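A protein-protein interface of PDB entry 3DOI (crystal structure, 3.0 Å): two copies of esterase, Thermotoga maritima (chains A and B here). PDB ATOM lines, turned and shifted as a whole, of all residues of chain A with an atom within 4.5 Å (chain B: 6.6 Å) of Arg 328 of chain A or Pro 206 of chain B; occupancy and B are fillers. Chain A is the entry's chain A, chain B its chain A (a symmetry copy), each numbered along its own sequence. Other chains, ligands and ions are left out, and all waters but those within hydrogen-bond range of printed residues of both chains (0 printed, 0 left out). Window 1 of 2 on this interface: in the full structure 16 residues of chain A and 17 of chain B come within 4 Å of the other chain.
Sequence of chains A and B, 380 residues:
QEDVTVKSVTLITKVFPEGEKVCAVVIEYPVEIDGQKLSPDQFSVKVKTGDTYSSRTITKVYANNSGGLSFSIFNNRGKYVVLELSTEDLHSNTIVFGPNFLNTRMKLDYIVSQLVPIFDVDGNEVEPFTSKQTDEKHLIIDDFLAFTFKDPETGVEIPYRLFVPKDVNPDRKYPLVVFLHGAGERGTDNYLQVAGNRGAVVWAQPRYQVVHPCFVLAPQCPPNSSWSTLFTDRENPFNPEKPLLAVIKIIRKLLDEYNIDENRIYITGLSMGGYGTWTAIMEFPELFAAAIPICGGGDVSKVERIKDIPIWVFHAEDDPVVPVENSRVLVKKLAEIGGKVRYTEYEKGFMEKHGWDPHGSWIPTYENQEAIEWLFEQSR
The guanidinium group (NH2) of Arg 207 of chain B lies within salt-bridge range of the side-chain carboxylate (OE2) of Glu 345 of chain A (3.6 Å).
The side-chain carboxylate of Glu 345 of chain A is in salt-bridge range of the guanidinium group of Arg 328 of chain A (2.6 Å).
The side-chain hydroxyl of Tyr 343 of chain A lies within hydrogen-bond range of the side-chain carboxylate of Glu 345 of chain A, 2.4 Å away.
Among the printed residues, merely in contact across the chains: Val 331 of chain A with Val 211 of chain B (3.2 Å), Lys 332 of chain A with Val 210 of chain B (3.3 Å), Arg 328 of chain A with Val 210 of chain B (3.3 Å), Arg 328 of chain A with Pro 206 of chain B (3.5 Å), Tyr 343 of chain A with Val 210 of chain B (3.8 Å), Val 331 of chain A with Val 210 of chain B (3.8 Å), Tyr 343 of chain A with Arg 207 of chain B (3.9 Å) and Glu 317 of chain A with Arg 207 of chain B (3.96 Å).
Pro 206 of chain B touches just one residue of chain A: Arg 328.
Printed residues of chain B within 4 Å of Lys 332 of chain A: Val 210.
Printed residues of chain A within 4 Å of Val 210 of chain B: Arg 328 (3.3 Å), Val 331 (3.8 Å), Lys 332 (3.3 Å) and Tyr 343 (3.8 Å).
Of the printed residues of chain B, Val 331 of chain A touches Val 210 (3.8 Å) and Val 211 (3.2 Å).
The nearest residue of chain B that does not touch Arg 328 of chain A is Arg 207 of chain B (4.6 Å).
Of the 11 printed residues of chain B, 4 touch a printed residue of chain A.
Hydrophobic or aromatic side chains of chain B within 4 Å of the printed part of chain A: Pro 206, Val 210 and Val 211.
Of the 12 printed residues of chain A, 6 touch a printed residue of chain B.
Hydrophobic or aromatic side chains of chain A that line the printed part of chain B: Val 331 and Tyr 343.
Among the printed residues, 9 pairs touch across the chains.
Among the printed residues, Asp or Glu carboxylates within 4 Å of a Lys or Arg side-chain nitrogen of the other chain: Glu 345 of chain A with Arg 207 of chain B (3.6 Å).
No position is printed for both chains.
Of the 9 pairs that touch across the chains among the printed residues, none has its exchanged pair printed and touching as well.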
ATOM      1  N   GLU A 317      -9.231   7.419  28.664  1.00  0.00           N
ATOM      2  CA  GLU A 317      -8.445   8.652  28.790  1.00  0.00           C
ATOM      3  C   GLU A 317      -9.264   9.807  29.390  1.00  0.00           C
ATOM      4  O   GLU A 317      -8.811  10.550  30.282  1.00  0.00           O
ATOM      5  CB  GLU A 317      -7.855   9.028  27.427  1.00  0.00           C
ATOM      6  CG  GLU A 317      -6.911  10.219  27.456  1.00  0.00           C
ATOM      7  CD  GLU A 317      -7.632  11.569  27.372  1.00  0.00           C
ATOM      8  OE1 GLU A 317      -8.887  11.631  27.376  1.00  0.00           O
ATOM      9  OE2 GLU A 317      -6.928  12.586  27.302  1.00  0.00           O
ATOM     10  N   VAL A 324      -7.566   9.604  34.702  1.00  0.00           N
ATOM     11  CA  VAL A 324      -6.783   8.542  34.054  1.00  0.00           C
ATOM     12  C   VAL A 324      -5.345   8.476  34.629  1.00  0.00           C
ATOM     13  O   VAL A 324      -4.717   7.395  34.674  1.00  0.00           O
ATOM     14  CB  VAL A 324      -6.856   8.628  32.486  1.00  0.00           C
ATOM     15  CG1 VAL A 324      -5.999   9.753  31.925  1.00  0.00           C
ATOM     16  CG2 VAL A 324      -6.465   7.328  31.851  1.00  0.00           C
ATOM     17  N   GLU A 325      -4.849   9.634  35.095  1.00  0.00           N
ATOM     18  CA  GLU A 325      -3.509   9.738  35.683  1.00  0.00           C
ATOM     19  C   GLU A 325      -3.324   8.689  36.807  1.00  0.00           C
ATOM     20  O   GLU A 325      -2.295   8.013  36.877  1.00  0.00           O
ATOM     21  CB  GLU A 325      -3.251  11.182  36.135  1.00  0.00           C
ATOM     22  CG  GLU A 325      -1.983  11.417  37.009  1.00  0.00           C
ATOM     23  CD  GLU A 325      -0.628  11.318  36.218  1.00  0.00           C
ATOM     24  OE1 GLU A 325      -0.566  10.692  35.107  1.00  0.00           O
ATOM     25  OE2 GLU A 325       0.389  11.871  36.735  1.00  0.00           O
ATOM     26  N   ASN A 326      -4.346   8.541  37.646  1.00  0.00           N
ATOM     27  CA  ASN A 326      -4.497   7.419  38.562  1.00  0.00           C
ATOM     28  C   ASN A 326      -4.000   6.015  38.101  1.00  0.00           C
ATOM     29  O   ASN A 326      -3.350   5.302  38.873  1.00  0.00           O
ATOM     30  CB  ASN A 326      -5.967   7.305  38.911  1.00  0.00           C
ATOM     31  CG  ASN A 326      -6.332   8.047  40.161  1.00  0.00           C
ATOM     32  OD1 ASN A 326      -6.168   7.529  41.257  1.00  0.00           O
ATOM     33  ND2 ASN A 326      -6.883   9.245  40.007  1.00  0.00           N
ATOM     34  N   SER A 327      -4.333   5.593  36.884  1.00  0.00           N
ATOM     35  CA  SER A 327      -3.847   4.301  36.378  1.00  0.00           C
ATOM     36  C   SER A 327      -2.456   4.414  35.784  1.00  0.00           C
ATOM     37  O   SER A 327      -1.695   3.450  35.787  1.00  0.00           O
ATOM     38  CB  SER A 327      -4.787   3.717  35.326  1.00  0.00           C
ATOM     39  OG  SER A 327      -5.824   2.974  35.929  1.00  0.00           O
ATOM     40  N   ARG A 328      -2.137   5.593  35.257  1.00  0.00           N
ATOM     41  CA  ARG A 328      -0.868   5.794  34.552  1.00  0.00           C
ATOM     42  C   ARG A 328       0.279   5.773  35.539  1.00  0.00           C
ATOM     43  O   ARG A 328       1.331   5.175  35.278  1.00  0.00           O
ATOM     44  CB  ARG A 328      -0.867   7.106  33.771  1.00  0.00           C
ATOM     45  CG  ARG A 328      -1.867   7.133  32.653  1.00  0.00           C
ATOM     46  CD  ARG A 328      -2.132   8.542  32.193  1.00  0.00           C
ATOM     47  NE  ARG A 328      -2.692   8.593  30.844  1.00  0.00           N
ATOM     48  CZ  ARG A 328      -2.848   9.714  30.163  1.00  0.00           C
ATOM     49  NH1 ARG A 328      -2.488  10.857  30.702  1.00  0.00           N
ATOM     50  NH2 ARG A 328      -3.360   9.696  28.956  1.00  0.00           N
ATOM     51  N   VAL A 329       0.041   6.417  36.684  1.00  0.00           N
ATOM     52  CA  VAL A 329       1.017   6.497  37.746  1.00  0.00           C
ATOM     53  C   VAL A 329       1.483   5.076  38.110  1.00  0.00           C
ATOM     54  O   VAL A 329       2.667   4.780  37.953  1.00  0.00           O
ATOM     55  CB  VAL A 329       0.482   7.345  38.932  1.00  0.00           C
ATOM     56  CG1 VAL A 329      -0.723   6.686  39.583  1.00  0.00           C
ATOM     57  CG2 VAL A 329       1.538   7.582  39.956  1.00  0.00           C
ATOM     58  N   LEU A 330       0.547   4.205  38.512  1.00  0.00           N
ATOM     59  CA  LEU A 330       0.820   2.791  38.773  1.00  0.00           C
ATOM     60  C   LEU A 330       1.522   2.046  37.629  1.00  0.00           C
ATOM     61  O   LEU A 330       2.595   1.459  37.829  1.00  0.00           O
ATOM     62  CB  LEU A 330      -0.461   2.036  39.104  1.00  0.00           C
ATOM     63  CG  LEU A 330      -1.051   2.106  40.499  1.00  0.00           C
ATOM     64  CD1 LEU A 330      -0.176   2.965  41.366  1.00  0.00           C
ATOM     65  CD2 LEU A 330      -2.417   2.698  40.424  1.00  0.00           C
ATOM     66  N   VAL A 331       0.917   2.046  36.440  1.00  0.00           N
ATOM     67  CA  VAL A 331       1.512   1.329  35.328  1.00  0.00           C
ATOM     68  C   VAL A 331       2.943   1.827  35.114  1.00  0.00           C
ATOM     69  O   VAL A 331       3.859   1.032  34.922  1.00  0.00           O
ATOM     70  CB  VAL A 331       0.730   1.510  34.033  1.00  0.00           C
ATOM     71  CG1 VAL A 331       1.453   0.827  32.888  1.00  0.00           C
ATOM     72  CG2 VAL A 331      -0.648   0.959  34.166  1.00  0.00           C
ATOM     73  N   LYS A 332       3.133   3.142  35.159  1.00  0.00           N
ATOM     74  CA  LYS A 332       4.439   3.711  34.849  1.00  0.00           C
ATOM     75  C   LYS A 332       5.425   3.155  35.828  1.00  0.00           C
ATOM     76  O   LYS A 332       6.451   2.607  35.424  1.00  0.00           O
ATOM     77  CB  LYS A 332       4.439   5.239  34.934  1.00  0.00           C
ATOM     78  CG  LYS A 332       5.724   5.937  34.474  1.00  0.00           C
ATOM     79  CD  LYS A 332       6.043   7.071  35.468  1.00  0.00           C
ATOM     80  CE  LYS A 332       6.896   8.184  34.858  1.00  0.00           C
ATOM     81  NZ  LYS A 332       8.155   7.634  34.240  1.00  0.00           N
ATOM     82  N   TYR A 343      -1.507  -2.626  29.553  1.00  0.00           N
ATOM     83  CA  TYR A 343      -2.267  -1.400  29.696  1.00  0.00           C
ATOM     84  C   TYR A 343      -2.883  -0.982  28.409  1.00  0.00           C
ATOM     85  O   TYR A 343      -2.187  -0.530  27.497  1.00  0.00           O
ATOM     86  CB  TYR A 343      -1.390  -0.256  30.216  1.00  0.00           C
ATOM     87  CG  TYR A 343      -2.139   1.012  30.530  1.00  0.00           C
ATOM     88  CD1 TYR A 343      -3.336   0.982  31.244  1.00  0.00           C
ATOM     89  CD2 TYR A 343      -1.635   2.244  30.141  1.00  0.00           C
ATOM     90  CE1 TYR A 343      -4.027   2.148  31.549  1.00  0.00           C
ATOM     91  CE2 TYR A 343      -2.308   3.436  30.440  1.00  0.00           C
ATOM     92  CZ  TYR A 343      -3.504   3.381  31.151  1.00  0.00           C
ATOM     93  OH  TYR A 343      -4.172   4.557  31.464  1.00  0.00           O
ATOM     94  N   GLU A 345      -5.351   1.857  27.408  1.00  0.00           N
ATOM     95  CA  GLU A 345      -6.026   3.103  27.757  1.00  0.00           C
ATOM     96  C   GLU A 345      -6.843   3.655  26.600  1.00  0.00           C
ATOM     97  O   GLU A 345      -6.266   4.201  25.652  1.00  0.00           O
ATOM     98  CB  GLU A 345      -5.005   4.143  28.134  1.00  0.00           C
ATOM     99  CG  GLU A 345      -5.637   5.460  28.481  1.00  0.00           C
ATOM    100  CD  GLU A 345      -4.638   6.518  28.880  1.00  0.00           C
ATOM    101  OE1 GLU A 345      -3.898   6.346  29.881  1.00  0.00           O
ATOM    102  OE2 GLU A 345      -4.613   7.545  28.186  1.00  0.00           O
ATOM    103  N   ILE B 140       0.874  17.123  22.321  1.00  0.00           N
ATOM    104  CA  ILE B 140       1.681  16.011  21.831  1.00  0.00           C
ATOM    105  C   ILE B 140       2.392  16.377  20.534  1.00  0.00           C
ATOM    106  O   ILE B 140       2.845  15.502  19.795  1.00  0.00           O
ATOM    107  CB  ILE B 140       0.826  14.751  21.601  1.00  0.00           C
ATOM    108  CG1 ILE B 140      -0.217  14.606  22.710  1.00  0.00           C
ATOM    109  CG2 ILE B 140       1.709  13.516  21.527  1.00  0.00           C
ATOM    110  CD1 ILE B 140       0.175  13.626  23.794  1.00  0.00           C
ATOM    111  N   VAL B 202       2.162   9.237  17.825  1.00  0.00           N
ATOM    112  CA  VAL B 202       1.567   8.061  18.501  1.00  0.00           C
ATOM    113  C   VAL B 202       2.497   7.512  19.581  1.00  0.00           C
ATOM    114  O   VAL B 202       2.070   7.182  20.699  1.00  0.00           O
ATOM    115  CB  VAL B 202       1.121   6.946  17.487  1.00  0.00           C
ATOM    116  CG1 VAL B 202       2.287   6.403  16.692  1.00  0.00           C
ATOM    117  CG2 VAL B 202       0.371   5.836  18.195  1.00  0.00           C
ATOM    118  N   TRP B 203       3.779   7.490  19.236  1.00  0.00           N
ATOM    119  CA  TRP B 203       4.774   6.837  20.019  1.00  0.00           C
ATOM    120  C   TRP B 203       5.014   7.681  21.212  1.00  0.00           C
ATOM    121  O   TRP B 203       5.644   7.243  22.159  1.00  0.00           O
ATOM    122  CB  TRP B 203       6.056   6.738  19.221  1.00  0.00           C
ATOM    123  CG  TRP B 203       5.855   6.120  17.878  1.00  0.00           C
ATOM    124  CD1 TRP B 203       5.860   6.765  16.677  1.00  0.00           C
ATOM    125  CD2 TRP B 203       5.598   4.740  17.595  1.00  0.00           C
ATOM    126  NE1 TRP B 203       5.622   5.867  15.664  1.00  0.00           N
ATOM    127  CE2 TRP B 203       5.459   4.620  16.205  1.00  0.00           C
ATOM    128  CE3 TRP B 203       5.467   3.602  18.383  1.00  0.00           C
ATOM    129  CZ2 TRP B 203       5.208   3.408  15.584  1.00  0.00           C
ATOM    130  CZ3 TRP B 203       5.208   2.397  17.771  1.00  0.00           C
ATOM    131  CH2 TRP B 203       5.079   2.307  16.386  1.00  0.00           C
ATOM    132  N   ALA B 204       4.519   8.908  21.174  1.00  0.00           N
ATOM    133  CA  ALA B 204       4.767   9.829  22.278  1.00  0.00           C
ATOM    134  C   ALA B 204       3.554   9.995  23.197  1.00  0.00           C
ATOM    135  O   ALA B 204       3.653  10.648  24.245  1.00  0.00           O
ATOM    136  CB  ALA B 204       5.261  11.162  21.764  1.00  0.00           C
ATOM    137  N   GLN B 205       2.431   9.386  22.817  1.00  0.00           N
ATOM    138  CA  GLN B 205       1.238   9.411  23.654  1.00  0.00           C
ATOM    139  C   GLN B 205       1.486   8.801  25.036  1.00  0.00           C
ATOM    140  O   GLN B 205       2.114   7.730  25.124  1.00  0.00           O
ATOM    141  CB  GLN B 205       0.120   8.656  22.966  1.00  0.00           C
ATOM    142  CG  GLN B 205      -0.679   9.522  22.063  1.00  0.00           C
ATOM    143  CD  GLN B 205      -1.565   8.721  21.136  1.00  0.00           C
ATOM    144  OE1 GLN B 205      -1.664   9.026  19.929  1.00  0.00           O
ATOM    145  NE2 GLN B 205      -2.219   7.693  21.684  1.00  0.00           N
ATOM    146  N   PRO B 206       1.029   9.485  26.121  1.00  0.00           N
ATOM    147  CA  PRO B 206       1.069   8.898  27.453  1.00  0.00           C
ATOM    148  C   PRO B 206       0.785   7.401  27.496  1.00  0.00           C
ATOM    149  O   PRO B 206       1.600   6.646  28.003  1.00  0.00           O
ATOM    150  CB  PRO B 206       0.027   9.713  28.205  1.00  0.00           C
ATOM    151  CG  PRO B 206       0.279  11.084  27.676  1.00  0.00           C
ATOM    152  CD  PRO B 206       0.528  10.873  26.195  1.00  0.00           C
ATOM    153  N   ARG B 207      -0.312   6.958  26.915  1.00  0.00           N
ATOM    154  CA  ARG B 207      -0.654   5.532  26.964  1.00  0.00           C
ATOM    155  C   ARG B 207       0.494   4.584  26.613  1.00  0.00           C
ATOM    156  O   ARG B 207       0.518   3.448  27.096  1.00  0.00           O
ATOM    157  CB  ARG B 207      -1.867   5.216  26.086  1.00  0.00           C
ATOM    158  CG  ARG B 207      -1.635   5.417  24.600  1.00  0.00           C
ATOM    159  CD  ARG B 207      -2.840   4.971  23.815  1.00  0.00           C
ATOM    160  NE  ARG B 207      -4.068   5.462  24.427  1.00  0.00           N
ATOM    161  CZ  ARG B 207      -4.596   6.644  24.160  1.00  0.00           C
ATOM    162  NH1 ARG B 207      -3.992   7.436  23.279  1.00  0.00           N
ATOM    163  NH2 ARG B 207      -5.716   7.031  24.765  1.00  0.00           N
ATOM    164  N   TYR B 208       1.433   5.025  25.786  1.00  0.00           N
ATOM    165  CA  TYR B 208       2.470   4.112  25.359  1.00  0.00           C
ATOM    166  C   TYR B 208       3.748   4.407  26.114  1.00  0.00           C
ATOM    167  O   TYR B 208       4.459   3.480  26.530  1.00  0.00           O
ATOM    168  CB  TYR B 208       2.660   4.098  23.808  1.00  0.00           C
ATOM    169  CG  TYR B 208       1.460   3.509  23.049  1.00  0.00           C
ATOM    170  CD1 TYR B 208       0.970   2.257  23.369  1.00  0.00           C
ATOM    171  CD2 TYR B 208       0.783   4.236  22.036  1.00  0.00           C
ATOM    172  CE1 TYR B 208      -0.138   1.728  22.697  1.00  0.00           C
ATOM    173  CE2 TYR B 208      -0.345   3.704  21.370  1.00  0.00           C
ATOM    174  CZ  TYR B 208      -0.784   2.454  21.710  1.00  0.00           C
ATOM    175  OH  TYR B 208      -1.863   1.864  21.108  1.00  0.00           O
ATOM    176  N   GLN B 209       4.016   5.699  26.309  1.00  0.00           N
ATOM    177  CA  GLN B 209       5.234   6.161  26.993  1.00  0.00           C
ATOM    178  C   GLN B 209       5.340   5.602  28.397  1.00  0.00           C
ATOM    179  O   GLN B 209       6.432   5.291  28.892  1.00  0.00           O
ATOM    180  CB  GLN B 209       5.282   7.680  27.056  1.00  0.00           C
ATOM    181  CG  GLN B 209       5.673   8.306  25.749  1.00  0.00           C
ATOM    182  CD  GLN B 209       7.117   8.039  25.386  1.00  0.00           C
ATOM    183  OE1 GLN B 209       7.969   7.857  26.259  1.00  0.00           O
ATOM    184  NE2 GLN B 209       7.407   8.038  24.087  1.00  0.00           N
ATOM    185  N   VAL B 210       4.176   5.474  29.018  1.00  0.00           N
ATOM    186  CA  VAL B 210       4.043   4.955  30.353  1.00  0.00           C
ATOM    187  C   VAL B 210       4.473   3.473  30.457  1.00  0.00           C
ATOM    188  O   VAL B 210       4.866   3.017  31.542  1.00  0.00           O
ATOM    189  CB  VAL B 210       2.612   5.174  30.821  1.00  0.00           C
ATOM    190  CG1 VAL B 210       1.766   3.899  30.617  1.00  0.00           C
ATOM    191  CG2 VAL B 210       2.590   5.669  32.246  1.00  0.00           C
ATOM    192  N   VAL B 211       4.428   2.743  29.339  1.00  0.00           N
ATOM    193  CA  VAL B 211       4.871   1.331  29.316  1.00  0.00           C
ATOM    194  C   VAL B 211       6.080   1.049  28.436  1.00  0.00           C
ATOM    195  O   VAL B 211       6.748   0.054  28.645  1.00  0.00           O
ATOM    196  CB  VAL B 211       3.732   0.301  28.984  1.00  0.00           C
ATOM    197  CG1 VAL B 211       2.651   0.371  30.006  1.00  0.00           C
ATOM    198  CG2 VAL B 211       3.136   0.530  27.601  1.00  0.00           C
